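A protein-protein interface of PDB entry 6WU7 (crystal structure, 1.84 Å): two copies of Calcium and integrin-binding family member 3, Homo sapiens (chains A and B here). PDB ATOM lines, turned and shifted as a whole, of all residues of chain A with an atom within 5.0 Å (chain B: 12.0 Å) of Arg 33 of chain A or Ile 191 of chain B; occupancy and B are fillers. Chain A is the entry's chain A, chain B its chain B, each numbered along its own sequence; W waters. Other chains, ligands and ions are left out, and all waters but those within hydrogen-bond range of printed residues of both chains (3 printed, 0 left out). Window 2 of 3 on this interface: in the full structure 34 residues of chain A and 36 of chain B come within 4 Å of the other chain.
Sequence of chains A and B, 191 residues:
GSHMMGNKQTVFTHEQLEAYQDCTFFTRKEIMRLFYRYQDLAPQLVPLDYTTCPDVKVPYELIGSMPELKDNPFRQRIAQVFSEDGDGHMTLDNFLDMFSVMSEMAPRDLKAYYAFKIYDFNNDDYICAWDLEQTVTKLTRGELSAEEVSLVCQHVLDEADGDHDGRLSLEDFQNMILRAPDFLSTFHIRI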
ATOM      1  N   LYS A  29     -20.894 -29.931  -6.012  1.00  0.00           N
ATOM      2  CA  LYS A  29     -21.381 -28.562  -6.204  1.00  0.00           C
ATOM      3  C   LYS A  29     -20.498 -27.558  -5.473  1.00  0.00           C
ATOM      4  O   LYS A  29     -20.190 -26.485  -6.012  1.00  0.00           O
ATOM      5  CB  LYS A  29     -22.843 -28.465  -5.733  1.00  0.00           C
ATOM      6  CG  LYS A  29     -23.334 -27.064  -5.333  1.00  0.00           C
ATOM      7  CD  LYS A  29     -24.462 -27.134  -4.270  1.00  0.00           C
ATOM      8  CE  LYS A  29     -25.464 -25.974  -4.368  1.00  0.00           C
ATOM      9  NZ  LYS A  29     -26.212 -25.726  -3.083  1.00  0.00           N
ATOM     10  N   GLU A  30     -20.063 -27.887  -4.249  1.00  0.00           N
ATOM     11  CA  GLU A  30     -19.194 -26.964  -3.531  1.00  0.00           C
ATOM     12  C   GLU A  30     -17.825 -26.863  -4.192  1.00  0.00           C
ATOM     13  O   GLU A  30     -17.256 -25.766  -4.296  1.00  0.00           O
ATOM     14  CB  GLU A  30     -19.079 -27.398  -2.070  1.00  0.00           C
ATOM     15  CG  GLU A  30     -20.397 -27.205  -1.342  1.00  0.00           C
ATOM     16  CD  GLU A  30     -20.483 -27.918  -0.001  1.00  0.00           C
ATOM     17  OE1 GLU A  30     -19.797 -28.942   0.214  1.00  0.00           O
ATOM     18  OE2 GLU A  30     -21.272 -27.444   0.839  1.00  0.00           O
ATOM     19  N   ILE A  31     -17.265 -27.990  -4.635  1.00  0.00           N
ATOM     20  CA  ILE A  31     -15.972 -27.943  -5.305  1.00  0.00           C
ATOM     21  C   ILE A  31     -16.039 -27.008  -6.496  1.00  0.00           C
ATOM     22  O   ILE A  31     -15.127 -26.192  -6.729  1.00  0.00           O
ATOM     23  CB  ILE A  31     -15.528 -29.362  -5.727  1.00  0.00           C
ATOM     24  CG1 ILE A  31     -15.279 -30.235  -4.483  1.00  0.00           C
ATOM     25  CG2 ILE A  31     -14.335 -29.259  -6.650  1.00  0.00           C
ATOM     26  CD1 ILE A  31     -14.214 -29.730  -3.616  1.00  0.00           C
ATOM     27  N   MET A  32     -17.124 -27.100  -7.268  1.00  0.00           N
ATOM     28  CA  MET A  32     -17.256 -26.259  -8.446  1.00  0.00           C
ATOM     29  C   MET A  32     -17.364 -24.787  -8.061  1.00  0.00           C
ATOM     30  O   MET A  32     -16.730 -23.933  -8.686  1.00  0.00           O
ATOM     31  CB  MET A  32     -18.465 -26.684  -9.262  1.00  0.00           C
ATOM     32  CG  MET A  32     -18.315 -28.043  -9.937  1.00  0.00           C
ATOM     33  SD  MET A  32     -16.816 -28.226 -10.911  1.00  0.00           S
ATOM     34  CE  MET A  32     -16.858 -26.731 -11.906  1.00  0.00           C
ATOM     35  N   ARG A  33     -18.145 -24.465  -7.031  1.00  0.00           N
ATOM     36  CA  ARG A  33     -18.252 -23.068  -6.620  1.00  0.00           C
ATOM     37  C   ARG A  33     -16.896 -22.525  -6.189  1.00  0.00           C
ATOM     38  O   ARG A  33     -16.521 -21.405  -6.550  1.00  0.00           O
ATOM     39  CB  ARG A  33     -19.249 -22.920  -5.475  1.00  0.00           C
ATOM     40  CG  ARG A  33     -19.291 -21.533  -4.842  1.00  0.00           C
ATOM     41  CD  ARG A  33     -20.501 -21.412  -3.905  1.00  0.00           C
ATOM     42  NE  ARG A  33     -20.230 -21.914  -2.557  1.00  0.00           N
ATOM     43  CZ  ARG A  33     -20.862 -22.943  -1.989  1.00  0.00           C
ATOM     44  NH1 ARG A  33     -21.804 -23.613  -2.648  1.00  0.00           N
ATOM     45  NH2 ARG A  33     -20.552 -23.311  -0.753  1.00  0.00           N
ATOM     46  N   LEU A  34     -16.148 -23.311  -5.420  1.00  0.00           N
ATOM     47  CA  LEU A  34     -14.870 -22.848  -4.920  1.00  0.00           C
ATOM     48  C   LEU A  34     -13.858 -22.728  -6.041  1.00  0.00           C
ATOM     49  O   LEU A  34     -12.971 -21.868  -5.994  1.00  0.00           O
ATOM     50  CB  LEU A  34     -14.361 -23.801  -3.843  1.00  0.00           C
ATOM     51  CG  LEU A  34     -14.878 -23.577  -2.423  1.00  0.00           C
ATOM     52  CD1 LEU A  34     -16.379 -23.443  -2.391  1.00  0.00           C
ATOM     53  CD2 LEU A  34     -14.416 -24.732  -1.537  1.00  0.00           C
ATOM     54  N   PHE A  35     -13.918 -23.628  -7.026  1.00  0.00           N
ATOM     55  CA  PHE A  35     -13.040 -23.473  -8.180  1.00  0.00           C
ATOM     56  C   PHE A  35     -13.237 -22.104  -8.811  1.00  0.00           C
ATOM     57  O   PHE A  35     -12.281 -21.403  -9.133  1.00  0.00           O
ATOM     58  CB  PHE A  35     -13.275 -24.525  -9.271  1.00  0.00           C
ATOM     59  CG  PHE A  35     -12.587 -24.133 -10.553  1.00  0.00           C
ATOM     60  CD1 PHE A  35     -11.207 -24.240 -10.652  1.00  0.00           C
ATOM     61  CD2 PHE A  35     -13.282 -23.543 -11.575  1.00  0.00           C
ATOM     62  CE1 PHE A  35     -10.545 -23.820 -11.784  1.00  0.00           C
ATOM     63  CE2 PHE A  35     -12.628 -23.116 -12.728  1.00  0.00           C
ATOM     64  CZ  PHE A  35     -11.240 -23.256 -12.825  1.00  0.00           C
ATOM     65  N   TYR A  36     -14.493 -21.719  -9.026  1.00  0.00           N
ATOM     66  CA  TYR A  36     -14.729 -20.454  -9.700  1.00  0.00           C
ATOM     67  C   TYR A  36     -14.304 -19.293  -8.822  1.00  0.00           C
ATOM     68  O   TYR A  36     -13.900 -18.244  -9.346  1.00  0.00           O
ATOM     69  CB  TYR A  36     -16.185 -20.388 -10.110  1.00  0.00           C
ATOM     70  CG  TYR A  36     -16.438 -21.199 -11.368  1.00  0.00           C
ATOM     71  CD1 TYR A  36     -15.914 -20.792 -12.595  1.00  0.00           C
ATOM     72  CD2 TYR A  36     -17.190 -22.361 -11.326  1.00  0.00           C
ATOM     73  CE1 TYR A  36     -16.140 -21.528 -13.748  1.00  0.00           C
ATOM     74  CE2 TYR A  36     -17.414 -23.106 -12.470  1.00  0.00           C
ATOM     75  CZ  TYR A  36     -16.884 -22.686 -13.674  1.00  0.00           C
ATOM     76  OH  TYR A  36     -17.116 -23.430 -14.822  1.00  0.00           O
ATOM     77  N   ARG A  37     -14.350 -19.457  -7.495  1.00  0.00           N
ATOM     78  CA  ARG A  37     -13.810 -18.408  -6.633  1.00  0.00           C
ATOM     79  C   ARG A  37     -12.304 -18.295  -6.812  1.00  0.00           C
ATOM     80  O   ARG A  37     -11.749 -17.196  -6.893  1.00  0.00           O
ATOM     81  CB  ARG A  37     -14.143 -18.695  -5.164  1.00  0.00           C
ATOM     82  CG  ARG A  37     -15.633 -18.505  -4.762  1.00  0.00           C
ATOM     83  CD  ARG A  37     -16.125 -17.083  -5.046  1.00  0.00           C
ATOM     84  NE  ARG A  37     -15.291 -16.073  -4.411  1.00  0.00           N
ATOM     85  CZ  ARG A  37     -15.367 -15.718  -3.136  1.00  0.00           C
ATOM     86  NH1 ARG A  37     -16.276 -16.250  -2.333  1.00  0.00           N
ATOM     87  NH2 ARG A  37     -14.550 -14.797  -2.651  1.00  0.00           N
ATOM     88  N   MET A  66      -8.623 -11.669  -0.610  1.00  0.00           N
ATOM     89  CA  MET A  66      -9.982 -12.091  -0.914  1.00  0.00           C
ATOM     90  C   MET A  66     -10.918 -11.754   0.249  1.00  0.00           C
ATOM     91  O   MET A  66     -10.483 -11.633   1.399  1.00  0.00           O
ATOM     92  CB  MET A  66     -10.009 -13.590  -1.243  1.00  0.00           C
ATOM     93  CG  MET A  66      -9.935 -14.546  -0.103  1.00  0.00           C
ATOM     94  SD  MET A  66      -9.858 -16.278  -0.725  1.00  0.00           S
ATOM     95  CE  MET A  66     -11.460 -16.541  -1.392  1.00  0.00           C
ATOM     96  N   GLU A  68     -13.007 -13.216   2.128  1.00  0.00           N
ATOM     97  CA  GLU A  68     -13.160 -14.139   3.242  1.00  0.00           C
ATOM     98  C   GLU A  68     -11.928 -14.198   4.137  1.00  0.00           C
ATOM     99  O   GLU A  68     -12.004 -14.760   5.238  1.00  0.00           O
ATOM    100  CB  GLU A  68     -13.442 -15.542   2.687  1.00  0.00           C
ATOM    101  CG  GLU A  68     -14.860 -15.720   2.171  1.00  0.00           C
ATOM    102  CD  GLU A  68     -15.062 -15.171   0.759  1.00  0.00           C
ATOM    103  OE1 GLU A  68     -14.083 -14.729   0.119  1.00  0.00           O
ATOM    104  OE2 GLU A  68     -16.222 -15.204   0.318  1.00  0.00           O
ATOM    105  N   PHE A  95      -5.734 -24.508  -2.132  1.00  0.00           N
ATOM    106  CA  PHE A  95      -6.878 -23.654  -1.818  1.00  0.00           C
ATOM    107  C   PHE A  95      -8.042 -24.475  -1.299  1.00  0.00           C
ATOM    108  O   PHE A  95      -8.693 -24.100  -0.316  1.00  0.00           O
ATOM    109  CB  PHE A  95      -7.243 -22.886  -3.099  1.00  0.00           C
ATOM    110  CG  PHE A  95      -8.424 -21.925  -3.002  1.00  0.00           C
ATOM    111  CD1 PHE A  95      -8.221 -20.601  -2.641  1.00  0.00           C
ATOM    112  CD2 PHE A  95      -9.687 -22.306  -3.421  1.00  0.00           C
ATOM    113  CE1 PHE A  95      -9.276 -19.702  -2.634  1.00  0.00           C
ATOM    114  CE2 PHE A  95     -10.741 -21.419  -3.423  1.00  0.00           C
ATOM    115  CZ  PHE A  95     -10.515 -20.102  -3.034  1.00  0.00           C
ATOM    116  N   PHE A  99      -9.742 -24.280   2.508  1.00  0.00           N
ATOM    117  CA  PHE A  99     -11.150 -24.025   2.803  1.00  0.00           C
ATOM    118  C   PHE A  99     -11.875 -25.267   3.291  1.00  0.00           C
ATOM    119  O   PHE A  99     -12.856 -25.128   4.031  1.00  0.00           O
ATOM    120  CB  PHE A  99     -11.762 -23.385   1.577  1.00  0.00           C
ATOM    121  CG  PHE A  99     -11.534 -21.893   1.547  1.00  0.00           C
ATOM    122  CD1 PHE A  99     -12.056 -21.097   2.547  1.00  0.00           C
ATOM    123  CD2 PHE A  99     -10.723 -21.308   0.572  1.00  0.00           C
ATOM    124  CE1 PHE A  99     -11.826 -19.725   2.559  1.00  0.00           C
ATOM    125  CE2 PHE A  99     -10.521 -19.915   0.580  1.00  0.00           C
ATOM    126  CZ  PHE A  99     -11.064 -19.144   1.573  1.00  0.00           C
ATOM    127  N   THR B 186     -10.733 -18.068  14.316  1.00  0.00           N
ATOM    128  CA  THR B 186     -10.197 -17.666  13.025  1.00  0.00           C
ATOM    129  C   THR B 186     -10.154 -18.825  12.037  1.00  0.00           C
ATOM    130  O   THR B 186      -9.724 -18.633  10.891  1.00  0.00           O
ATOM    131  CB  THR B 186      -8.809 -17.040  13.217  1.00  0.00           C
ATOM    132  OG1 THR B 186      -8.090 -17.760  14.215  1.00  0.00           O
ATOM    133  CG2 THR B 186      -8.961 -15.578  13.688  1.00  0.00           C
ATOM    134  N   PHE B 187     -10.657 -20.005  12.431  1.00  0.00           N
ATOM    135  CA  PHE B 187     -10.684 -21.191  11.581  1.00  0.00           C
ATOM    136  C   PHE B 187     -12.101 -21.584  11.169  1.00  0.00           C
ATOM    137  O   PHE B 187     -12.344 -22.746  10.824  1.00  0.00           O
ATOM    138  CB  PHE B 187      -9.978 -22.346  12.290  1.00  0.00           C
ATOM    139  CG  PHE B 187      -8.521 -22.136  12.358  1.00  0.00           C
ATOM    140  CD1 PHE B 187      -7.701 -22.740  11.437  1.00  0.00           C
ATOM    141  CD2 PHE B 187      -7.980 -21.240  13.277  1.00  0.00           C
ATOM    142  CE1 PHE B 187      -6.357 -22.502  11.431  1.00  0.00           C
ATOM    143  CE2 PHE B 187      -6.603 -20.986  13.274  1.00  0.00           C
ATOM    144  CZ  PHE B 187      -5.809 -21.611  12.341  1.00  0.00           C
ATOM    145  N   HIS B 188     -13.044 -20.640  11.194  1.00  0.00           N
ATOM    146  CA  HIS B 188     -14.399 -20.875  10.701  1.00  0.00           C
ATOM    147  C   HIS B 188     -14.612 -19.869   9.584  1.00  0.00           C
ATOM    148  O   HIS B 188     -14.885 -18.694   9.839  1.00  0.00           O
ATOM    149  CB  HIS B 188     -15.431 -20.736  11.795  1.00  0.00           C
ATOM    150  CG  HIS B 188     -15.505 -21.949  12.669  1.00  0.00           C
ATOM    151  ND1 HIS B 188     -14.865 -22.019  13.888  1.00  0.00           N
ATOM    152  CD2 HIS B 188     -16.126 -23.141  12.491  1.00  0.00           C
ATOM    153  CE1 HIS B 188     -15.100 -23.194  14.437  1.00  0.00           C
ATOM    154  NE2 HIS B 188     -15.869 -23.893  13.616  1.00  0.00           N
ATOM    155  N   ILE B 189     -14.423 -20.316   8.352  1.00  0.00           N
ATOM    156  CA  ILE B 189     -14.469 -19.431   7.190  1.00  0.00           C
ATOM    157  C   ILE B 189     -15.339 -20.116   6.156  1.00  0.00           C
ATOM    158  O   ILE B 189     -14.920 -21.116   5.555  1.00  0.00           O
ATOM    159  CB  ILE B 189     -13.087 -19.136   6.612  1.00  0.00           C
ATOM    160  CG1 ILE B 189     -12.083 -18.797   7.718  1.00  0.00           C
ATOM    161  CG2 ILE B 189     -13.184 -17.971   5.629  1.00  0.00           C
ATOM    162  CD1 ILE B 189     -10.685 -18.437   7.205  1.00  0.00           C
ATOM    163  N   ARG B 190     -16.540 -19.580   5.938  1.00  0.00           N
ATOM    164  CA  ARG B 190     -17.464 -20.157   4.976  1.00  0.00           C
ATOM    165  C   ARG B 190     -17.261 -19.526   3.598  1.00  0.00           C
ATOM    166  O   ARG B 190     -16.996 -18.325   3.471  1.00  0.00           O
ATOM    167  CB  ARG B 190     -18.901 -19.975   5.428  1.00  0.00           C
ATOM    168  CG  ARG B 190     -19.327 -20.801   6.647  1.00  0.00           C
ATOM    169  CD  ARG B 190     -20.734 -20.388   7.126  1.00  0.00           C
ATOM    170  NE  ARG B 190     -21.165 -19.121   6.528  1.00  0.00           N
ATOM    171  CZ  ARG B 190     -22.278 -18.945   5.821  1.00  0.00           C
ATOM    172  NH1 ARG B 190     -23.124 -19.946   5.618  1.00  0.00           N
ATOM    173  NH2 ARG B 190     -22.550 -17.750   5.316  1.00  0.00           N
ATOM    174  N   ILE B 191     -17.414 -20.349   2.570  1.00  0.00           N
ATOM    175  CA  ILE B 191     -17.262 -19.931   1.188  1.00  0.00           C
ATOM    176  C   ILE B 191     -18.144 -20.828   0.322  1.00  0.00           C
ATOM    177  O   ILE B 191     -18.703 -21.803   0.829  1.00  0.00           O
ATOM    178  CB  ILE B 191     -15.805 -19.988   0.787  1.00  0.00           C
ATOM    179  CG1 ILE B 191     -15.582 -19.274  -0.531  1.00  0.00           C
ATOM    180  CG2 ILE B 191     -15.339 -21.425   0.704  1.00  0.00           C
ATOM    181  CD1 ILE B 191     -14.159 -18.924  -0.748  1.00  0.00           C
ATOM    182  OXT ILE B 191     -18.362 -20.583  -0.875  1.00  0.00           O
HETATM  183  O   HOH W   1     -18.365 -18.303  -2.455  1.00  0.00           O
HETATM  184  O   HOH W   2     -18.246 -16.325   1.789  1.00  0.00           O
HETATM  185  O   HOH W   3     -14.852 -23.181   3.981  1.00  0.00           O
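Arg 33 of chain A touches just one residue of chain B: Ile 191. No residue of chain B comes within 4 Å of Lys 29 of chain A. No residue of chain B comes within 4 Å of Glu 30 of chain A. No residue of chain B comes within 4 Å of Ile 31 of chain A. Of the printed residues of chain B, Leu 34 of chain A touches Ile 191. No residue of chain B comes within 4 Å of Tyr 36 of chain A. Of chain B, only Ile 191 (3.6 Å) comes within 4 Å of Arg 37 of chain A. Of the printed residues of chain B, Glu 68 of chain A touches Ile 189 and Arg 190. Of chain B, only Ile 189 and Ile 191 come within 4 Å of Phe 99 of chain A. Printed residues of chain B within 4 Å of Met 66 of chain A: Ile 191 (3.7 Å). Printed residues of chain A within 4 Å of Ile 189 of chain B: Glu 68 (3.4 Å) and Phe 99 (3.8 Å). Phe 35 of chain A touches none of the printed residues of chain B. The nearest residue of chain B that does not touch Arg 33 of chain A is Arg 190 of chain B (6.6 Å). The nearest residue of chain A that does not touch Ile 191 of chain B is Glu 68 of chain A (4.1 Å).
Ile 191 of chain B touches Leu 34 of chain A (OXT to CD1, 3.8 Å). CG1 of Ile 191 of chain B touches NH1 of Arg 37 of chain A, 3.6 Å away. Ile 191 of chain B touches Met 66 of chain A (CD1 to CE, 3.7 Å). Glu 68 of chain A touches Ile 189 of chain B (O to CG2, 3.4 Å). Glu 68 of chain A touches Arg 190 of chain B. CE1 of Phe 99 of chain A touches CG2 of Ile 189 of chain B, 3.8 Å away. CD1 of Phe 99 of chain A touches CG2 of Ile 191 of chain B, 3.8 Å away.
No position is printed for both chains. Of the 8 pairs that touch across the chains among the printed residues, none has its exchanged pair printed and touching as well.
The guanidinium group (NE) of Arg 33 of chain A lies within salt-bridge range of the chain-end carboxylate (OXT) of Ile 191 of chain B (2.8 Å).
Hydrophobic or aromatic side chains of chain B that line the printed part of chain A: Ile 189 and Ile 191. Printed residues of chain A that touch a printed residue of chain B: Arg 33, Leu 34, Arg 37, Met 66, Glu 68 and Phe 99. Hydrophobic or aromatic side chains of chain A within 4 Å of the printed part of chain B: Leu 34, Met 66 and Phe 99. Among the printed residues, no Asp or Glu carboxylate lies within 4 Å of a Lys or Arg side-chain nitrogen of the other chain.
Water W3 bridges O of Ile 189 of chain B (2.6 Å) and O of Phe 99 of chain A (2.8 Å). Water W2 lies within hydrogen-bond range of OE2 of Glu 68 of chain A (2.7 Å) and O of Arg 190 of chain B (2.9 Å). Water W1 bridges OXT of Ile 191 of chain B and NH1 of Arg 37 of chain A.
NH2 of Arg 37 of chain A lies within salt-bridge range of OE1 of Glu 68 of chain A (2.8 Å).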
